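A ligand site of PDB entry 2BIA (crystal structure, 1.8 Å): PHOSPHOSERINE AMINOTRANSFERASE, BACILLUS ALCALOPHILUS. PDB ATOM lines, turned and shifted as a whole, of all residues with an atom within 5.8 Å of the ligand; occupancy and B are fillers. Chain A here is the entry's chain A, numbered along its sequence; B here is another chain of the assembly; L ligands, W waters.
NZ of Lys 196 is covalently linked to C5 of the ligand (1.5 Å).
An oxygen (O1) of the ligand lies within hydrogen-bond range of the side-chain hydroxyl (OG1) of Thr 152 (2.5 Å).
N of Ser 77 lies within hydrogen-bond range of O4 of the ligand (2.8 Å).
OG of Ser 77 sits at hydrogen-bond distance from O4 of the ligand, at 2.7 Å.
OD2 of Asp 172 is in hydrogen-bond range of N1 of the ligand, 2.7 Å away.
An oxygen (O3) of the ligand sits at hydrogen-bond distance from the backbone NH (N) of Thr 238 of chain B (3.0 Å).
O3 of the ligand lies within hydrogen-bond range of OG1 of Thr 238 of chain B, at 2.7 Å.
The side-chain amide nitrogen (NE2) of Gln 195 lies within hydrogen-bond range of an oxygen (O5) of the ligand (2.9 Å).
An oxygen (O4) of the ligand is in hydrogen-bond range of the side-chain amide nitrogen of Asn 237 of chain B (3.0 Å).
N of Ala 76 lies within hydrogen-bond range of O5 of the ligand, at 3.3 Å.
The indole nitrogen (NE1) of Trp 102 lies close to an oxygen (O1) of the ligand, 3.5 Å away.
The side-chain hydroxyl of Thr 152 sits at hydrogen-bond distance from the side-chain hydroxyl of Ser 175, at 2.8 Å.
The side-chain carboxylate of Asp 172 is in hydrogen-bond range of the side-chain hydroxyl of Ser 174 (2.8 Å).
The side-chain hydroxyl (OG1) of Thr 238 of chain B lies within hydrogen-bond range of the side-chain amide nitrogen (NE2) of Gln 195 (3.2 Å).
The backbone carbonyl oxygen of Thr 238 of chain B sits at hydrogen-bond distance from the side-chain amide nitrogen of Gln 73 of chain B.
ND2 of Asn 237 of chain B is in hydrogen-bond range of O of Gly 74 (3.3 Å).
The side-chain hydroxyl (OG1) of Thr 204 sits close to the backbone NH (N) of Gly 75 (3.1 Å).
OG of Ser 174 sits at hydrogen-bond distance from N of Gly 193 (3.3 Å).
OD1 of Asn 150 sits at hydrogen-bond distance from OG of Ser 175 (2.9 Å).
Water W3 lies within hydrogen-bond range of the backbone carbonyl oxygen of Thr 238 of chain B (2.7 Å), an oxygen (O5) of the ligand (2.8 Å), the side-chain amide nitrogen of Gln 73 of chain B (3.1 Å) and the side-chain amide nitrogen of Asn 237 of chain B (3.5 Å).
Water W1 lies within hydrogen-bond range of O2 of the ligand (2.8 Å), OG of Ser 174 (3.0 Å), N of Gly 193 (3.2 Å) and NE2 of Gln 195 (3.5 Å).
CA of Gly 75 touches O5 of the ligand, at 3.3 Å.
CZ of Phe 80 touches C7 of the ligand, 3.7 Å away.
O of Asn 150 touches C2 of the ligand, at 3.8 Å.
Ser 174 touches the ligand (CB to C1, 3.5 Å).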
ATOM      1  N   GLY A  74      -9.566 -35.689 -15.080  1.00  0.00           N
ATOM      2  CA  GLY A  74     -10.281 -34.741 -14.234  1.00  0.00           C
ATOM      3  C   GLY A  74      -9.719 -33.339 -14.314  1.00  0.00           C
ATOM      4  O   GLY A  74     -10.336 -32.395 -13.807  1.00  0.00           O
ATOM      5  N   GLY A  75      -8.565 -33.203 -14.966  1.00  0.00           N
ATOM      6  CA  GLY A  75      -8.013 -31.868 -15.113  1.00  0.00           C
ATOM      7  C   GLY A  75      -7.338 -31.367 -13.849  1.00  0.00           C
ATOM      8  O   GLY A  75      -7.337 -31.962 -12.773  1.00  0.00           O
ATOM      9  N   ALA A  76      -6.711 -30.187 -14.021  1.00  0.00           N
ATOM     10  CA  ALA A  76      -6.101 -29.541 -12.866  1.00  0.00           C
ATOM     11  C   ALA A  76      -7.174 -29.224 -11.838  1.00  0.00           C
ATOM     12  O   ALA A  76      -6.975 -29.240 -10.631  1.00  0.00           O
ATOM     13  CB  ALA A  76      -5.352 -28.293 -13.305  1.00  0.00           C
ATOM     14  N   SER A  77      -8.360 -28.922 -12.363  1.00  0.00           N
ATOM     15  CA  SER A  77      -9.468 -28.566 -11.459  1.00  0.00           C
ATOM     16  C   SER A  77      -9.761 -29.656 -10.456  1.00  0.00           C
ATOM     17  O   SER A  77     -10.038 -29.356  -9.288  1.00  0.00           O
ATOM     18  CB  SER A  77     -10.730 -28.216 -12.261  1.00  0.00           C
ATOM     19  OG  SER A  77     -10.485 -27.003 -12.967  1.00  0.00           O
ATOM     20  N   LEU A  78      -9.697 -30.923 -10.875  1.00  0.00           N
ATOM     21  CA  LEU A  78      -9.900 -31.984  -9.917  1.00  0.00           C
ATOM     22  C   LEU A  78      -8.763 -32.033  -8.891  1.00  0.00           C
ATOM     23  O   LEU A  78      -8.984 -32.380  -7.729  1.00  0.00           O
ATOM     24  CB  LEU A  78     -10.015 -33.366 -10.584  1.00  0.00           C
ATOM     25  CG  LEU A  78     -10.291 -34.493  -9.583  1.00  0.00           C
ATOM     26  CD1 LEU A  78     -11.528 -34.169  -8.755  1.00  0.00           C
ATOM     27  CD2 LEU A  78     -10.457 -35.846 -10.283  1.00  0.00           C
ATOM     28  N   PHE A  80      -7.318 -29.532  -7.611  1.00  0.00           N
ATOM     29  CA  PHE A  80      -7.649 -28.512  -6.609  1.00  0.00           C
ATOM     30  C   PHE A  80      -8.332 -29.129  -5.398  1.00  0.00           C
ATOM     31  O   PHE A  80      -8.156 -28.704  -4.254  1.00  0.00           O
ATOM     32  CB  PHE A  80      -8.542 -27.423  -7.201  1.00  0.00           C
ATOM     33  CG  PHE A  80      -7.929 -26.521  -8.258  1.00  0.00           C
ATOM     34  CD1 PHE A  80      -8.766 -25.750  -9.057  1.00  0.00           C
ATOM     35  CD2 PHE A  80      -6.553 -26.445  -8.450  1.00  0.00           C
ATOM     36  CE1 PHE A  80      -8.263 -24.888 -10.041  1.00  0.00           C
ATOM     37  CE2 PHE A  80      -6.043 -25.587  -9.399  1.00  0.00           C
ATOM     38  CZ  PHE A  80      -6.881 -24.822 -10.190  1.00  0.00           C
ATOM     39  N   TRP A 102      -6.386 -18.637 -11.051  1.00  0.00           N
ATOM     40  CA  TRP A 102      -6.261 -20.071 -10.803  1.00  0.00           C
ATOM     41  C   TRP A 102      -5.811 -20.329  -9.368  1.00  0.00           C
ATOM     42  O   TRP A 102      -6.243 -21.302  -8.746  1.00  0.00           O
ATOM     43  CB  TRP A 102      -5.329 -20.738 -11.828  1.00  0.00           C
ATOM     44  CG  TRP A 102      -5.983 -20.751 -13.190  1.00  0.00           C
ATOM     45  CD1 TRP A 102      -5.571 -20.113 -14.321  1.00  0.00           C
ATOM     46  CD2 TRP A 102      -7.170 -21.467 -13.548  1.00  0.00           C
ATOM     47  NE1 TRP A 102      -6.429 -20.369 -15.371  1.00  0.00           N
ATOM     48  CE2 TRP A 102      -7.424 -21.209 -14.901  1.00  0.00           C
ATOM     49  CE3 TRP A 102      -8.045 -22.308 -12.839  1.00  0.00           C
ATOM     50  CZ2 TRP A 102      -8.518 -21.758 -15.591  1.00  0.00           C
ATOM     51  CZ3 TRP A 102      -9.126 -22.830 -13.518  1.00  0.00           C
ATOM     52  CH2 TRP A 102      -9.368 -22.568 -14.867  1.00  0.00           C
ATOM     53  N   THR A 148       0.980 -21.220  -7.755  1.00  0.00           N
ATOM     54  CA  THR A 148       0.689 -21.309  -9.181  1.00  0.00           C
ATOM     55  C   THR A 148       1.883 -20.764  -9.953  1.00  0.00           C
ATOM     56  O   THR A 148       2.095 -19.551  -9.972  1.00  0.00           O
ATOM     57  CB  THR A 148      -0.595 -20.551  -9.496  1.00  0.00           C
ATOM     58  OG1 THR A 148      -1.554 -20.944  -8.492  1.00  0.00           O
ATOM     59  CG2 THR A 148      -1.156 -20.904 -10.862  1.00  0.00           C
ATOM     60  N   ASN A 150       2.759 -20.452 -13.136  1.00  0.00           N
ATOM     61  CA  ASN A 150       2.397 -19.543 -14.228  1.00  0.00           C
ATOM     62  C   ASN A 150       0.916 -19.193 -14.143  1.00  0.00           C
ATOM     63  O   ASN A 150       0.017 -20.048 -14.149  1.00  0.00           O
ATOM     64  CB  ASN A 150       2.761 -20.142 -15.598  1.00  0.00           C
ATOM     65  CG  ASN A 150       2.560 -19.145 -16.721  1.00  0.00           C
ATOM     66  OD1 ASN A 150       1.533 -19.177 -17.406  1.00  0.00           O
ATOM     67  ND2 ASN A 150       3.501 -18.249 -16.947  1.00  0.00           N
ATOM     68  N   ASN A 151       0.647 -17.880 -14.027  1.00  0.00           N
ATOM     69  CA  ASN A 151      -0.721 -17.407 -13.810  1.00  0.00           C
ATOM     70  C   ASN A 151      -1.356 -17.059 -15.153  1.00  0.00           C
ATOM     71  O   ASN A 151      -1.225 -15.946 -15.643  1.00  0.00           O
ATOM     72  CB  ASN A 151      -0.700 -16.205 -12.847  1.00  0.00           C
ATOM     73  CG  ASN A 151       0.048 -16.608 -11.587  1.00  0.00           C
ATOM     74  OD1 ASN A 151      -0.528 -17.244 -10.700  1.00  0.00           O
ATOM     75  ND2 ASN A 151       1.313 -16.257 -11.497  1.00  0.00           N
ATOM     76  N   THR A 152      -2.004 -18.080 -15.701  1.00  0.00           N
ATOM     77  CA  THR A 152      -2.381 -18.125 -17.100  1.00  0.00           C
ATOM     78  C   THR A 152      -3.207 -16.925 -17.547  1.00  0.00           C
ATOM     79  O   THR A 152      -3.148 -16.470 -18.689  1.00  0.00           O
ATOM     80  CB  THR A 152      -3.214 -19.409 -17.361  1.00  0.00           C
ATOM     81  OG1 THR A 152      -2.657 -20.422 -16.537  1.00  0.00           O
ATOM     82  CG2 THR A 152      -3.078 -19.850 -18.807  1.00  0.00           C
ATOM     83  N   ASP A 172       0.783 -25.774  -8.951  1.00  0.00           N
ATOM     84  CA  ASP A 172       0.000 -25.886 -10.173  1.00  0.00           C
ATOM     85  C   ASP A 172       0.864 -25.373 -11.321  1.00  0.00           C
ATOM     86  O   ASP A 172       0.981 -24.147 -11.493  1.00  0.00           O
ATOM     87  CB  ASP A 172      -1.298 -25.103 -10.049  1.00  0.00           C
ATOM     88  CG  ASP A 172      -2.144 -25.087 -11.292  1.00  0.00           C
ATOM     89  OD1 ASP A 172      -1.732 -25.705 -12.314  1.00  0.00           O
ATOM     90  OD2 ASP A 172      -3.232 -24.454 -11.240  1.00  0.00           O
ATOM     91  N   MET A 173       1.441 -26.284 -12.113  1.00  0.00           N
ATOM     92  CA  MET A 173       2.242 -25.817 -13.265  1.00  0.00           C
ATOM     93  C   MET A 173       1.564 -26.038 -14.602  1.00  0.00           C
ATOM     94  O   MET A 173       2.274 -26.184 -15.594  1.00  0.00           O
ATOM     95  CB  MET A 173       3.587 -26.529 -13.252  1.00  0.00           C
ATOM     96  CG  MET A 173       4.407 -26.235 -11.998  1.00  0.00           C
ATOM     97  SD  MET A 173       6.107 -26.810 -12.226  1.00  0.00           S
ATOM     98  CE  MET A 173       6.858 -26.184 -10.704  1.00  0.00           C
ATOM     99  N   SER A 174       0.235 -26.054 -14.651  1.00  0.00           N
ATOM    100  CA  SER A 174      -0.525 -26.333 -15.862  1.00  0.00           C
ATOM    101  C   SER A 174      -0.011 -25.568 -17.061  1.00  0.00           C
ATOM    102  O   SER A 174       0.157 -26.121 -18.159  1.00  0.00           O
ATOM    103  CB  SER A 174      -2.008 -26.007 -15.644  1.00  0.00           C
ATOM    104  OG  SER A 174      -2.579 -26.875 -14.657  1.00  0.00           O
ATOM    105  N   SER A 175       0.264 -24.250 -16.891  1.00  0.00           N
ATOM    106  CA  SER A 175       0.610 -23.527 -18.127  1.00  0.00           C
ATOM    107  C   SER A 175       2.092 -23.276 -18.311  1.00  0.00           C
ATOM    108  O   SER A 175       2.401 -22.516 -19.241  1.00  0.00           O
ATOM    109  CB  SER A 175      -0.189 -22.215 -18.214  1.00  0.00           C
ATOM    110  OG  SER A 175      -0.141 -21.501 -16.983  1.00  0.00           O
ATOM    111  N   TYR A 191       1.500 -30.491 -10.342  1.00  0.00           N
ATOM    112  CA  TYR A 191       0.463 -31.031 -11.236  1.00  0.00           C
ATOM    113  C   TYR A 191       0.237 -30.076 -12.394  1.00  0.00           C
ATOM    114  O   TYR A 191       0.489 -28.883 -12.298  1.00  0.00           O
ATOM    115  CB  TYR A 191      -0.804 -31.327 -10.453  1.00  0.00           C
ATOM    116  CG  TYR A 191      -1.494 -30.151  -9.808  1.00  0.00           C
ATOM    117  CD1 TYR A 191      -2.487 -29.437 -10.463  1.00  0.00           C
ATOM    118  CD2 TYR A 191      -1.146 -29.738  -8.517  1.00  0.00           C
ATOM    119  CE1 TYR A 191      -3.120 -28.361  -9.879  1.00  0.00           C
ATOM    120  CE2 TYR A 191      -1.789 -28.663  -7.923  1.00  0.00           C
ATOM    121  CZ  TYR A 191      -2.767 -27.982  -8.601  1.00  0.00           C
ATOM    122  OH  TYR A 191      -3.417 -26.903  -8.042  1.00  0.00           O
ATOM    123  N   GLY A 193      -2.629 -29.873 -15.941  1.00  0.00           N
ATOM    124  CA  GLY A 193      -3.436 -30.450 -17.022  1.00  0.00           C
ATOM    125  C   GLY A 193      -2.538 -30.458 -18.258  1.00  0.00           C
ATOM    126  O   GLY A 193      -1.747 -29.533 -18.514  1.00  0.00           O
ATOM    127  N   GLN A 195      -3.173 -30.047 -21.429  1.00  0.00           N
ATOM    128  CA  GLN A 195      -3.616 -29.354 -22.636  1.00  0.00           C
ATOM    129  C   GLN A 195      -2.975 -27.997 -22.821  1.00  0.00           C
ATOM    130  O   GLN A 195      -3.266 -27.261 -23.775  1.00  0.00           O
ATOM    131  CB  GLN A 195      -5.136 -29.197 -22.618  1.00  0.00           C
ATOM    132  CG  GLN A 195      -5.639 -28.233 -21.548  1.00  0.00           C
ATOM    133  CD  GLN A 195      -5.925 -28.936 -20.226  1.00  0.00           C
ATOM    134  OE1 GLN A 195      -5.437 -30.036 -19.949  1.00  0.00           O
ATOM    135  NE2 GLN A 195      -6.716 -28.280 -19.389  1.00  0.00           N
ATOM    136  N   LYS A 196      -2.077 -27.545 -21.945  1.00  0.00           N
ATOM    137  CA  LYS A 196      -1.533 -26.230 -22.338  1.00  0.00           C
ATOM    138  C   LYS A 196      -0.178 -26.394 -22.978  1.00  0.00           C
ATOM    139  O   LYS A 196       0.185 -25.847 -24.018  1.00  0.00           O
ATOM    140  CB  LYS A 196      -1.510 -25.296 -21.127  1.00  0.00           C
ATOM    141  CG  LYS A 196      -2.736 -25.463 -20.251  1.00  0.00           C
ATOM    142  CD  LYS A 196      -3.127 -24.166 -19.571  1.00  0.00           C
ATOM    143  CE  LYS A 196      -4.627 -23.950 -19.671  1.00  0.00           C
ATOM    144  NZ  LYS A 196      -5.274 -23.785 -18.338  1.00  0.00           N
ATOM    145  N   THR A 204      -4.059 -35.360 -16.917  1.00  0.00           N
ATOM    146  CA  THR A 204      -3.428 -34.470 -15.964  1.00  0.00           C
ATOM    147  C   THR A 204      -2.158 -35.132 -15.446  1.00  0.00           C
ATOM    148  O   THR A 204      -2.244 -36.262 -14.966  1.00  0.00           O
ATOM    149  CB  THR A 204      -4.374 -34.140 -14.785  1.00  0.00           C
ATOM    150  OG1 THR A 204      -5.467 -33.387 -15.315  1.00  0.00           O
ATOM    151  CG2 THR A 204      -3.678 -33.264 -13.760  1.00  0.00           C
ATOM    152  N   TYR A 338       2.930 -21.042 -25.767  1.00  0.00           N
ATOM    153  CA  TYR A 338       3.429 -22.289 -25.222  1.00  0.00           C
ATOM    154  C   TYR A 338       4.508 -22.908 -26.118  1.00  0.00           C
ATOM    155  O   TYR A 338       4.700 -22.420 -27.223  1.00  0.00           O
ATOM    156  CB  TYR A 338       2.272 -23.274 -25.061  1.00  0.00           C
ATOM    157  CG  TYR A 338       1.163 -22.781 -24.165  1.00  0.00           C
ATOM    158  CD1 TYR A 338      -0.127 -22.636 -24.671  1.00  0.00           C
ATOM    159  CD2 TYR A 338       1.385 -22.453 -22.838  1.00  0.00           C
ATOM    160  CE1 TYR A 338      -1.148 -22.175 -23.867  1.00  0.00           C
ATOM    161  CE2 TYR A 338       0.363 -21.998 -22.027  1.00  0.00           C
ATOM    162  CZ  TYR A 338      -0.907 -21.854 -22.544  1.00  0.00           C
ATOM    163  OH  TYR A 338      -1.966 -21.414 -21.774  1.00  0.00           O
ATOM    164  N   HIS B  41     -11.646 -25.067 -25.878  1.00  0.00           N
ATOM    165  CA  HIS B  41     -12.954 -25.627 -25.588  1.00  0.00           C
ATOM    166  C   HIS B  41     -14.000 -24.525 -25.507  1.00  0.00           C
ATOM    167  O   HIS B  41     -15.195 -24.794 -25.437  1.00  0.00           O
ATOM    168  CB  HIS B  41     -12.912 -26.438 -24.282  1.00  0.00           C
ATOM    169  CG  HIS B  41     -12.527 -25.634 -23.088  1.00  0.00           C
ATOM    170  ND1 HIS B  41     -11.314 -24.993 -22.966  1.00  0.00           N
ATOM    171  CD2 HIS B  41     -13.211 -25.376 -21.941  1.00  0.00           C
ATOM    172  CE1 HIS B  41     -11.266 -24.357 -21.795  1.00  0.00           C
ATOM    173  NE2 HIS B  41     -12.417 -24.587 -21.154  1.00  0.00           N
ATOM    174  N   GLN B  73     -15.057 -36.674 -16.887  1.00  0.00           N
ATOM    175  CA  GLN B  73     -13.845 -37.461 -16.844  1.00  0.00           C
ATOM    176  C   GLN B  73     -13.861 -38.369 -15.621  1.00  0.00           C
ATOM    177  O   GLN B  73     -14.730 -38.168 -14.753  1.00  0.00           O
ATOM    178  CB  GLN B  73     -12.631 -36.522 -16.768  1.00  0.00           C
ATOM    179  CG  GLN B  73     -12.468 -35.582 -17.978  1.00  0.00           C
ATOM    180  CD  GLN B  73     -11.179 -34.780 -17.811  1.00  0.00           C
ATOM    181  OE1 GLN B  73     -10.079 -35.351 -17.825  1.00  0.00           O
ATOM    182  NE2 GLN B  73     -11.335 -33.469 -17.635  1.00  0.00           N
ATOM    183  N   ASN B 237     -14.829 -27.009 -16.588  1.00  0.00           N
ATOM    184  CA  ASN B 237     -13.394 -26.995 -16.849  1.00  0.00           C
ATOM    185  C   ASN B 237     -13.163 -27.585 -18.238  1.00  0.00           C
ATOM    186  O   ASN B 237     -14.096 -27.766 -19.018  1.00  0.00           O
ATOM    187  CB  ASN B 237     -12.567 -27.710 -15.803  1.00  0.00           C
ATOM    188  CG  ASN B 237     -12.698 -29.207 -15.795  1.00  0.00           C
ATOM    189  OD1 ASN B 237     -13.768 -29.764 -16.067  1.00  0.00           O
ATOM    190  ND2 ASN B 237     -11.577 -29.851 -15.482  1.00  0.00           N
ATOM    191  N   THR B 238     -11.918 -27.844 -18.554  1.00  0.00           N
ATOM    192  CA  THR B 238     -11.605 -28.301 -19.919  1.00  0.00           C
ATOM    193  C   THR B 238     -12.081 -29.739 -20.077  1.00  0.00           C
ATOM    194  O   THR B 238     -11.612 -30.620 -19.347  1.00  0.00           O
ATOM    195  CB  THR B 238     -10.090 -28.207 -20.212  1.00  0.00           C
ATOM    196  OG1 THR B 238      -9.582 -26.922 -19.828  1.00  0.00           O
ATOM    197  CG2 THR B 238      -9.820 -28.370 -21.707  1.00  0.00           C
HETATM  198  N1  LIG L   1      -4.652 -24.178 -13.494  1.00  0.00           N
HETATM  199  C1  LIG L   1      -4.063 -23.396 -14.443  1.00  0.00           C
HETATM  200  C2  LIG L   1      -2.805 -22.590 -14.122  1.00  0.00           C
HETATM  201  C3  LIG L   1      -4.631 -23.317 -15.686  1.00  0.00           C
HETATM  202  O1  LIG L   1      -3.999 -22.524 -16.610  1.00  0.00           O
HETATM  203  C4  LIG L   1      -5.816 -23.980 -15.938  1.00  0.00           C
HETATM  204  C5  LIG L   1      -6.414 -23.955 -17.367  1.00  0.00           C
HETATM  205  C6  LIG L   1      -6.372 -24.808 -15.009  1.00  0.00           C
HETATM  206  C7  LIG L   1      -5.801 -24.880 -13.760  1.00  0.00           C
HETATM  207  C8  LIG L   1      -7.643 -25.635 -15.296  1.00  0.00           C
HETATM  208  O2  LIG L   1      -7.356 -26.899 -15.857  1.00  0.00           O
HETATM  209  P1  LIG L   1      -8.536 -27.929 -16.257  1.00  0.00           P
HETATM  210  O3  LIG L   1      -9.360 -27.118 -17.165  1.00  0.00           O
HETATM  211  O4  LIG L   1      -9.150 -28.220 -14.936  1.00  0.00           O
HETATM  212  O5  LIG L   1      -7.821 -29.057 -16.874  1.00  0.00           O
HETATM  213  O   HOH W   1      -4.747 -27.607 -16.603  1.00  0.00           O
HETATM  214  O   HOH W   2     -10.852 -24.957 -16.866  1.00  0.00           O
HETATM  215  O   HOH W   3      -9.397 -31.057 -17.924  1.00  0.00           O
